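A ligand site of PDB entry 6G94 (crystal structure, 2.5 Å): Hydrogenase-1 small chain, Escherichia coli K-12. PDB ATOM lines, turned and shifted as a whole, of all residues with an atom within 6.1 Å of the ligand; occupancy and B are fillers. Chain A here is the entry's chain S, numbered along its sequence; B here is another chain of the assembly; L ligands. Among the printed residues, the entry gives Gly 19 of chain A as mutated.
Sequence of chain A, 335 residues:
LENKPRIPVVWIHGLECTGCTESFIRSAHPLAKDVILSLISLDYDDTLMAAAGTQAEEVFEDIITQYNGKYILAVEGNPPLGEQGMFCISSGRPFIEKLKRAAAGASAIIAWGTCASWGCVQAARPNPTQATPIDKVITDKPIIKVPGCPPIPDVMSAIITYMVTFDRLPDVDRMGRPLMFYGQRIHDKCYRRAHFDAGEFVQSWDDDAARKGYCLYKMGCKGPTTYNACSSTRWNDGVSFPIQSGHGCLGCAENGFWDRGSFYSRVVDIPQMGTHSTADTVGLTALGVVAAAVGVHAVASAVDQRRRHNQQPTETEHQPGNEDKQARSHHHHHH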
ATOM      1  N   LEU A  15     -20.989   6.247  -2.827  1.00  0.00           N
ATOM      2  CA  LEU A  15     -20.808   5.405  -3.995  1.00  0.00           C
ATOM      3  C   LEU A  15     -20.311   6.297  -5.071  1.00  0.00           C
ATOM      4  O   LEU A  15     -20.961   7.258  -5.397  1.00  0.00           O
ATOM      5  CB  LEU A  15     -22.100   4.712  -4.386  1.00  0.00           C
ATOM      6  CG  LEU A  15     -22.515   3.530  -3.498  1.00  0.00           C
ATOM      7  CD1 LEU A  15     -23.901   3.050  -3.864  1.00  0.00           C
ATOM      8  CD2 LEU A  15     -21.491   2.391  -3.518  1.00  0.00           C
ATOM      9  N   GLU A  16     -19.118   6.002  -5.593  1.00  0.00           N
ATOM     10  CA  GLU A  16     -18.506   6.872  -6.589  1.00  0.00           C
ATOM     11  C   GLU A  16     -17.414   6.156  -7.338  1.00  0.00           C
ATOM     12  O   GLU A  16     -17.182   4.965  -7.077  1.00  0.00           O
ATOM     13  CB  GLU A  16     -17.964   8.134  -5.918  1.00  0.00           C
ATOM     14  CG  GLU A  16     -17.407   7.900  -4.527  1.00  0.00           C
ATOM     15  CD  GLU A  16     -15.896   8.045  -4.496  1.00  0.00           C
ATOM     16  OE1 GLU A  16     -15.451   9.102  -4.009  1.00  0.00           O
ATOM     17  OE2 GLU A  16     -15.166   7.152  -4.988  1.00  0.00           O
ATOM     18  N   CYS A  17     -16.781   6.857  -8.272  1.00  0.00           N
ATOM     19  CA  CYS A  17     -15.683   6.298  -9.085  1.00  0.00           C
ATOM     20  C   CYS A  17     -14.374   6.992  -8.760  1.00  0.00           C
ATOM     21  O   CYS A  17     -13.312   6.631  -9.304  1.00  0.00           O
ATOM     22  CB  CYS A  17     -15.944   6.330 -10.600  1.00  0.00           C
ATOM     23  SG  CYS A  17     -15.606   7.891 -11.457  1.00  0.00           S
ATOM     24  N   THR A  18     -14.468   7.983  -7.876  1.00  0.00           N
ATOM     25  CA  THR A  18     -13.337   8.819  -7.461  1.00  0.00           C
ATOM     26  C   THR A  18     -12.793   9.667  -8.642  1.00  0.00           C
ATOM     27  O   THR A  18     -11.697  10.245  -8.565  1.00  0.00           O
ATOM     28  CB  THR A  18     -12.189   7.990  -6.795  1.00  0.00           C
ATOM     29  OG1 THR A  18     -12.753   6.953  -5.990  1.00  0.00           O
ATOM     30  CG2 THR A  18     -11.324   8.854  -5.940  1.00  0.00           C
ATOM     31  N   GLY A  19     -13.571   9.754  -9.734  1.00  0.00           N
ATOM     32  CA  GLY A  19     -13.246  10.675 -10.807  1.00  0.00           C
ATOM     33  C   GLY A  19     -13.257  12.155 -10.405  1.00  0.00           C
ATOM     34  O   GLY A  19     -12.484  12.943 -10.941  1.00  0.00           O
ATOM     35  N   CYS A  20     -14.117  12.533  -9.469  1.00  0.00           N
ATOM     36  CA  CYS A  20     -14.239  13.920  -9.028  1.00  0.00           C
ATOM     37  C   CYS A  20     -13.004  14.337  -8.235  1.00  0.00           C
ATOM     38  O   CYS A  20     -12.465  15.416  -8.476  1.00  0.00           O
ATOM     39  CB  CYS A  20     -15.541  14.140  -8.226  1.00  0.00           C
ATOM     40  SG  CYS A  20     -17.104  13.930  -9.155  1.00  0.00           S
ATOM     41  N   THR A  21     -12.563  13.484  -7.312  1.00  0.00           N
ATOM     42  CA  THR A  21     -11.309  13.707  -6.593  1.00  0.00           C
ATOM     43  C   THR A  21     -10.132  13.824  -7.580  1.00  0.00           C
ATOM     44  O   THR A  21      -9.300  14.719  -7.460  1.00  0.00           O
ATOM     45  CB  THR A  21     -11.031  12.580  -5.555  1.00  0.00           C
ATOM     46  OG1 THR A  21     -11.855  12.788  -4.403  1.00  0.00           O
ATOM     47  CG2 THR A  21      -9.544  12.554  -5.146  1.00  0.00           C
ATOM     48  N   GLU A  76     -18.493  13.657  -2.311  1.00  0.00           N
ATOM     49  CA  GLU A  76     -18.289  12.986  -3.573  1.00  0.00           C
ATOM     50  C   GLU A  76     -19.060  11.672  -3.502  1.00  0.00           C
ATOM     51  O   GLU A  76     -19.069  11.020  -2.468  1.00  0.00           O
ATOM     52  CB  GLU A  76     -16.810  12.767  -3.790  1.00  0.00           C
ATOM     53  CG  GLU A  76     -16.462  12.164  -5.123  1.00  0.00           C
ATOM     54  CD  GLU A  76     -14.971  12.179  -5.346  1.00  0.00           C
ATOM     55  OE1 GLU A  76     -14.532  11.604  -6.362  1.00  0.00           O
ATOM     56  OE2 GLU A  76     -14.237  12.750  -4.515  1.00  0.00           O
ATOM     57  N   GLY A  77     -19.719  11.288  -4.589  1.00  0.00           N
ATOM     58  CA  GLY A  77     -20.593  10.112  -4.578  1.00  0.00           C
ATOM     59  C   GLY A  77     -21.934  10.323  -3.892  1.00  0.00           C
ATOM     60  O   GLY A  77     -22.294  11.458  -3.542  1.00  0.00           O
ATOM     61  N   TRP A 112     -20.095  17.540  -5.137  1.00  0.00           N
ATOM     62  CA  TRP A 112     -19.210  17.371  -6.294  1.00  0.00           C
ATOM     63  C   TRP A 112     -19.789  16.383  -7.308  1.00  0.00           C
ATOM     64  O   TRP A 112     -20.212  15.294  -6.937  1.00  0.00           O
ATOM     65  CB  TRP A 112     -17.807  16.882  -5.880  1.00  0.00           C
ATOM     66  CG  TRP A 112     -16.947  17.853  -5.130  1.00  0.00           C
ATOM     67  CD1 TRP A 112     -16.359  17.632  -3.926  1.00  0.00           C
ATOM     68  CD2 TRP A 112     -16.556  19.171  -5.538  1.00  0.00           C
ATOM     69  NE1 TRP A 112     -15.618  18.725  -3.554  1.00  0.00           N
ATOM     70  CE2 TRP A 112     -15.723  19.696  -4.526  1.00  0.00           C
ATOM     71  CE3 TRP A 112     -16.833  19.970  -6.656  1.00  0.00           C
ATOM     72  CZ2 TRP A 112     -15.164  20.979  -4.589  1.00  0.00           C
ATOM     73  CZ3 TRP A 112     -16.278  21.243  -6.720  1.00  0.00           C
ATOM     74  CH2 TRP A 112     -15.441  21.736  -5.693  1.00  0.00           C
ATOM     75  N   GLY A 113     -19.794  16.783  -8.577  1.00  0.00           N
ATOM     76  CA  GLY A 113     -20.133  15.898  -9.678  1.00  0.00           C
ATOM     77  C   GLY A 113     -21.595  15.523  -9.801  1.00  0.00           C
ATOM     78  O   GLY A 113     -22.424  15.886  -8.953  1.00  0.00           O
ATOM     79  N   THR A 114     -21.905  14.790 -10.868  1.00  0.00           N
ATOM     80  CA  THR A 114     -23.252  14.308 -11.153  1.00  0.00           C
ATOM     81  C   THR A 114     -23.762  13.301 -10.112  1.00  0.00           C
ATOM     82  O   THR A 114     -24.932  13.309  -9.772  1.00  0.00           O
ATOM     83  CB  THR A 114     -23.301  13.715 -12.566  1.00  0.00           C
ATOM     84  OG1 THR A 114     -22.958  14.752 -13.497  1.00  0.00           O
ATOM     85  CG2 THR A 114     -24.694  13.152 -12.896  1.00  0.00           C
ATOM     86  N   CYS A 115     -22.868  12.440  -9.612  1.00  0.00           N
ATOM     87  CA  CYS A 115     -23.176  11.547  -8.484  1.00  0.00           C
ATOM     88  C   CYS A 115     -23.887  12.241  -7.312  1.00  0.00           C
ATOM     89  O   CYS A 115     -25.044  11.918  -7.004  1.00  0.00           O
ATOM     90  CB  CYS A 115     -21.897  10.886  -7.972  1.00  0.00           C
ATOM     91  SG  CYS A 115     -21.347   9.519  -8.968  1.00  0.00           S
ATOM     92  N   ALA A 116     -23.198  13.180  -6.680  1.00  0.00           N
ATOM     93  CA  ALA A 116     -23.732  13.876  -5.505  1.00  0.00           C
ATOM     94  C   ALA A 116     -24.892  14.786  -5.871  1.00  0.00           C
ATOM     95  O   ALA A 116     -25.846  14.959  -5.090  1.00  0.00           O
ATOM     96  CB  ALA A 116     -22.636  14.662  -4.788  1.00  0.00           C
ATOM     97  N   CYS A 120     -26.055  10.077 -11.092  1.00  0.00           N
ATOM     98  CA  CYS A 120     -25.098   9.581 -12.095  1.00  0.00           C
ATOM     99  C   CYS A 120     -25.292   8.090 -12.426  1.00  0.00           C
ATOM    100  O   CYS A 120     -26.415   7.562 -12.307  1.00  0.00           O
ATOM    101  CB  CYS A 120     -23.656   9.888 -11.679  1.00  0.00           C
ATOM    102  SG  CYS A 120     -22.488  10.060 -13.042  1.00  0.00           S
ATOM    103  N   VAL A 121     -24.221   7.417 -12.817  1.00  0.00           N
ATOM    104  CA  VAL A 121     -24.297   6.095 -13.429  1.00  0.00           C
ATOM    105  C   VAL A 121     -24.958   5.013 -12.565  1.00  0.00           C
ATOM    106  O   VAL A 121     -25.695   4.184 -13.077  1.00  0.00           O
ATOM    107  CB  VAL A 121     -22.891   5.616 -13.896  1.00  0.00           C
ATOM    108  CG1 VAL A 121     -21.991   5.244 -12.718  1.00  0.00           C
ATOM    109  CG2 VAL A 121     -23.020   4.475 -14.920  1.00  0.00           C
ATOM    110  N   GLN A 122     -24.695   5.017 -11.255  1.00  0.00           N
ATOM    111  CA  GLN A 122     -25.283   4.014 -10.377  1.00  0.00           C
ATOM    112  C   GLN A 122     -26.792   4.199 -10.236  1.00  0.00           C
ATOM    113  O   GLN A 122     -27.513   3.243  -9.862  1.00  0.00           O
ATOM    114  CB  GLN A 122     -24.646   4.049  -8.992  1.00  0.00           C
ATOM    115  CG  GLN A 122     -24.626   5.407  -8.331  1.00  0.00           C
ATOM    116  CD  GLN A 122     -23.280   6.081  -8.451  1.00  0.00           C
ATOM    117  OE1 GLN A 122     -22.583   5.941  -9.461  1.00  0.00           O
ATOM    118  NE2 GLN A 122     -22.897   6.815  -7.419  1.00  0.00           N
ATOM    119  N   GLY A 148     -21.467  17.318 -13.513  1.00  0.00           N
ATOM    120  CA  GLY A 148     -20.472  16.926 -14.499  1.00  0.00           C
ATOM    121  C   GLY A 148     -19.903  15.601 -14.082  1.00  0.00           C
ATOM    122  O   GLY A 148     -19.906  15.256 -12.890  1.00  0.00           O
ATOM    123  N   CYS A 149     -19.398  14.839 -15.048  1.00  0.00           N
ATOM    124  CA  CYS A 149     -18.831  13.510 -14.774  1.00  0.00           C
ATOM    125  C   CYS A 149     -17.411  13.326 -15.332  1.00  0.00           C
ATOM    126  O   CYS A 149     -17.220  12.679 -16.365  1.00  0.00           O
ATOM    127  CB  CYS A 149     -19.769  12.406 -15.303  1.00  0.00           C
ATOM    128  SG  CYS A 149     -19.395  10.748 -14.683  1.00  0.00           S
ATOM    129  N   PRO A 150     -16.398  13.906 -14.657  1.00  0.00           N
ATOM    130  CA  PRO A 150     -16.485  14.806 -13.491  1.00  0.00           C
ATOM    131  C   PRO A 150     -16.655  16.279 -13.920  1.00  0.00           C
ATOM    132  O   PRO A 150     -16.620  16.590 -15.115  1.00  0.00           O
ATOM    133  CB  PRO A 150     -15.152  14.583 -12.805  1.00  0.00           C
ATOM    134  CG  PRO A 150     -14.209  14.305 -13.934  1.00  0.00           C
ATOM    135  CD  PRO A 150     -15.001  13.598 -15.009  1.00  0.00           C
ATOM    136  N   PRO A 151     -16.855  17.198 -12.948  1.00  0.00           N
ATOM    137  CA  PRO A 151     -16.778  18.603 -13.324  1.00  0.00           C
ATOM    138  C   PRO A 151     -15.386  18.973 -13.848  1.00  0.00           C
ATOM    139  O   PRO A 151     -14.418  18.225 -13.603  1.00  0.00           O
ATOM    140  CB  PRO A 151     -17.064  19.342 -12.018  1.00  0.00           C
ATOM    141  CG  PRO A 151     -17.567  18.339 -11.063  1.00  0.00           C
ATOM    142  CD  PRO A 151     -17.100  17.005 -11.510  1.00  0.00           C
ATOM    143  N   PHE A 257     -28.787  11.838 -17.269  1.00  0.00           N
ATOM    144  CA  PHE A 257     -28.371  11.876 -18.669  1.00  0.00           C
ATOM    145  C   PHE A 257     -28.090  10.495 -19.226  1.00  0.00           C
ATOM    146  O   PHE A 257     -28.111  10.287 -20.440  1.00  0.00           O
ATOM    147  CB  PHE A 257     -27.144  12.781 -18.853  1.00  0.00           C
ATOM    148  CG  PHE A 257     -25.859  12.147 -18.399  1.00  0.00           C
ATOM    149  CD1 PHE A 257     -25.501  12.155 -17.071  1.00  0.00           C
ATOM    150  CD2 PHE A 257     -25.007  11.545 -19.328  1.00  0.00           C
ATOM    151  CE1 PHE A 257     -24.326  11.566 -16.661  1.00  0.00           C
ATOM    152  CE2 PHE A 257     -23.832  10.956 -18.919  1.00  0.00           C
ATOM    153  CZ  PHE A 257     -23.482  10.978 -17.576  1.00  0.00           C
ATOM    154  N   TRP A 258     -27.804   9.554 -18.337  1.00  0.00           N
ATOM    155  CA  TRP A 258     -27.525   8.158 -18.722  1.00  0.00           C
ATOM    156  C   TRP A 258     -28.762   7.519 -19.389  1.00  0.00           C
ATOM    157  O   TRP A 258     -28.622   6.703 -20.311  1.00  0.00           O
ATOM    158  CB  TRP A 258     -27.118   7.330 -17.497  1.00  0.00           C
ATOM    159  CG  TRP A 258     -25.821   7.725 -16.895  1.00  0.00           C
ATOM    160  CD1 TRP A 258     -25.634   8.394 -15.716  1.00  0.00           C
ATOM    161  CD2 TRP A 258     -24.499   7.485 -17.430  1.00  0.00           C
ATOM    162  NE1 TRP A 258     -24.288   8.593 -15.490  1.00  0.00           N
ATOM    163  CE2 TRP A 258     -23.568   8.032 -16.519  1.00  0.00           C
ATOM    164  CE3 TRP A 258     -24.021   6.856 -18.592  1.00  0.00           C
ATOM    165  CZ2 TRP A 258     -22.191   7.975 -16.739  1.00  0.00           C
ATOM    166  CZ3 TRP A 258     -22.657   6.804 -18.810  1.00  0.00           C
ATOM    167  CH2 TRP A 258     -21.754   7.353 -17.882  1.00  0.00           C
ATOM    168  N   ARG B  54     -22.165  -0.870  -6.810  1.00  0.00           N
ATOM    169  CA  ARG B  54     -23.026  -0.025  -7.669  1.00  0.00           C
ATOM    170  C   ARG B  54     -23.889  -0.809  -8.666  1.00  0.00           C
ATOM    171  O   ARG B  54     -25.089  -0.525  -8.833  1.00  0.00           O
ATOM    172  CB  ARG B  54     -22.178   1.028  -8.382  1.00  0.00           C
ATOM    173  CG  ARG B  54     -21.745   2.170  -7.481  1.00  0.00           C
ATOM    174  CD  ARG B  54     -20.612   2.990  -8.082  1.00  0.00           C
ATOM    175  NE  ARG B  54     -19.475   2.160  -8.474  1.00  0.00           N
ATOM    176  CZ  ARG B  54     -18.575   2.502  -9.395  1.00  0.00           C
ATOM    177  NH1 ARG B  54     -18.675   3.657 -10.025  1.00  0.00           N
ATOM    178  NH2 ARG B  54     -17.588   1.682  -9.708  1.00  0.00           N
ATOM    179  N   ARG B  74     -17.065   4.709 -16.168  1.00  0.00           N
ATOM    180  CA  ARG B  74     -17.401   5.231 -14.837  1.00  0.00           C
ATOM    181  C   ARG B  74     -17.305   4.182 -13.716  1.00  0.00           C
ATOM    182  O   ARG B  74     -17.609   4.490 -12.560  1.00  0.00           O
ATOM    183  CB  ARG B  74     -18.787   5.900 -14.861  1.00  0.00           C
ATOM    184  CG  ARG B  74     -18.765   7.381 -15.252  1.00  0.00           C
ATOM    185  CD  ARG B  74     -18.372   7.600 -16.706  1.00  0.00           C
ATOM    186  NE  ARG B  74     -18.358   9.009 -17.103  1.00  0.00           N
ATOM    187  CZ  ARG B  74     -18.153   9.464 -18.351  1.00  0.00           C
ATOM    188  NH1 ARG B  74     -17.952   8.630 -19.365  1.00  0.00           N
ATOM    189  NH2 ARG B  74     -18.139  10.771 -18.572  1.00  0.00           N
ATOM    190  N   GLY B  77     -12.678   6.236 -11.817  1.00  0.00           N
ATOM    191  CA  GLY B  77     -12.068   7.495 -12.248  1.00  0.00           C
ATOM    192  C   GLY B  77     -10.553   7.557 -12.069  1.00  0.00           C
ATOM    193  O   GLY B  77      -9.870   8.435 -12.638  1.00  0.00           O
ATOM    194  N   PRO B 228     -10.487  13.425 -16.118  1.00  0.00           N
ATOM    195  CA  PRO B 228     -10.862  12.017 -16.224  1.00  0.00           C
ATOM    196  C   PRO B 228     -11.990  11.722 -17.226  1.00  0.00           C
ATOM    197  O   PRO B 228     -12.696  12.626 -17.639  1.00  0.00           O
ATOM    198  CB  PRO B 228     -11.291  11.673 -14.768  1.00  0.00           C
ATOM    199  CG  PRO B 228     -10.628  12.697 -13.912  1.00  0.00           C
ATOM    200  CD  PRO B 228     -10.699  13.940 -14.757  1.00  0.00           C
ATOM    201  N   HIS B 229     -12.092  10.451 -17.615  1.00  0.00           N
ATOM    202  CA  HIS B 229     -13.164   9.900 -18.461  1.00  0.00           C
ATOM    203  C   HIS B 229     -13.172  10.425 -19.893  1.00  0.00           C
ATOM    204  O   HIS B 229     -14.149  11.052 -20.322  1.00  0.00           O
ATOM    205  CB  HIS B 229     -14.527  10.119 -17.794  1.00  0.00           C
ATOM    206  CG  HIS B 229     -14.696   9.402 -16.481  1.00  0.00           C
ATOM    207  ND1 HIS B 229     -14.062   8.209 -16.191  1.00  0.00           N
ATOM    208  CD2 HIS B 229     -15.461   9.692 -15.391  1.00  0.00           C
ATOM    209  CE1 HIS B 229     -14.430   7.798 -14.990  1.00  0.00           C
ATOM    210  NE2 HIS B 229     -15.277   8.686 -14.478  1.00  0.00           N
HETATM  211  S1  LIG L   1     -19.780  12.156 -10.960  1.00  0.00           S
HETATM  212 FE1  LIG L   1     -20.262  10.545 -12.527  1.00  0.00          FE
HETATM  213 FE2  LIG L   1     -17.543  11.988 -10.394  1.00  0.00          FE
HETATM  214  S2  LIG L   1     -16.517  11.118 -12.267  1.00  0.00           S
HETATM  215  S3  LIG L   1     -17.499  10.283  -8.853  1.00  0.00           S
HETATM  216 FE3  LIG L   1     -17.158   9.395 -10.947  1.00  0.00          FE
HETATM  217 FE4  LIG L   1     -19.475  10.118  -9.938  1.00  0.00          FE
HETATM  218  S4  LIG L   1     -19.191   8.671 -11.675  1.00  0.00           S
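The side-chain sulfur of Cys 115 is bound to an iron atom (FE4) of the ligand, at 2.2 Å.
The side-chain sulfur of Cys 149 is bound to an iron atom (FE1) of the ligand, at 2.3 Å.
S2 of the ligand sits close to NE2 of His 229 of chain B.
FE2 of the ligand is bound by SG of Cys 20.
FE3 of the ligand is bound by SG of Cys 17.
The backbone NH (N) of Cys 115 lies close to a sulfur (S1) of the ligand.
A sulfur (S3) of the ligand lies close to the backbone NH (N) of Cys 17, at 3.5 Å.
The side-chain sulfur of Cys 120 binds an iron atom (FE1) of the ligand.
The backbone NH of Thr 114 lies close to a sulfur (S1) of the ligand (3.4 Å).
O of Gly 148 lies close to S1 of the ligand, 3.7 Å away.
N of Pro 150 lies close to S2 of the ligand, at 3.7 Å.
Residues that only touch the ligand: Gly 19 (3.6 Å), Glu 16 (3.7 Å), Arg 74 of chain B (3.8 Å), Thr 18 (3.9 Å) and Gly 113 (3.97 Å).
The nearest printed residue that does not touch the ligand is Glu 76 (4.1 Å).
The side-chain sulfur of Cys 17 sits close to a ring nitrogen (NE2) of His 229 of chain B (3.1 Å).
The backbone carbonyl oxygen (O) of Cys 149 lies within hydrogen-bond range of the guanidinium group (NH2) of Arg 74 of chain B.
SG of Cys 120 lies close to NE1 of Trp 258 (3.4 Å).
The backbone carbonyl oxygen of Arg 74 of chain B is in hydrogen-bond range of the guanidinium group of Arg 54 of chain B.
O of Cys 17 sits at hydrogen-bond distance from N of Gly 77 of chain B, 2.6 Å away.
N of Thr 114 lies within hydrogen-bond range of O of Gly 148, at 2.9 Å.
The side-chain hydroxyl (OG1) of Thr 18 sits at hydrogen-bond distance from the side-chain carboxylate (OE2) of Glu 16, at 2.6 Å.
The side-chain sulfur of Cys 115 sits close to the side-chain amide nitrogen of Gln 122 (3.5 Å).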
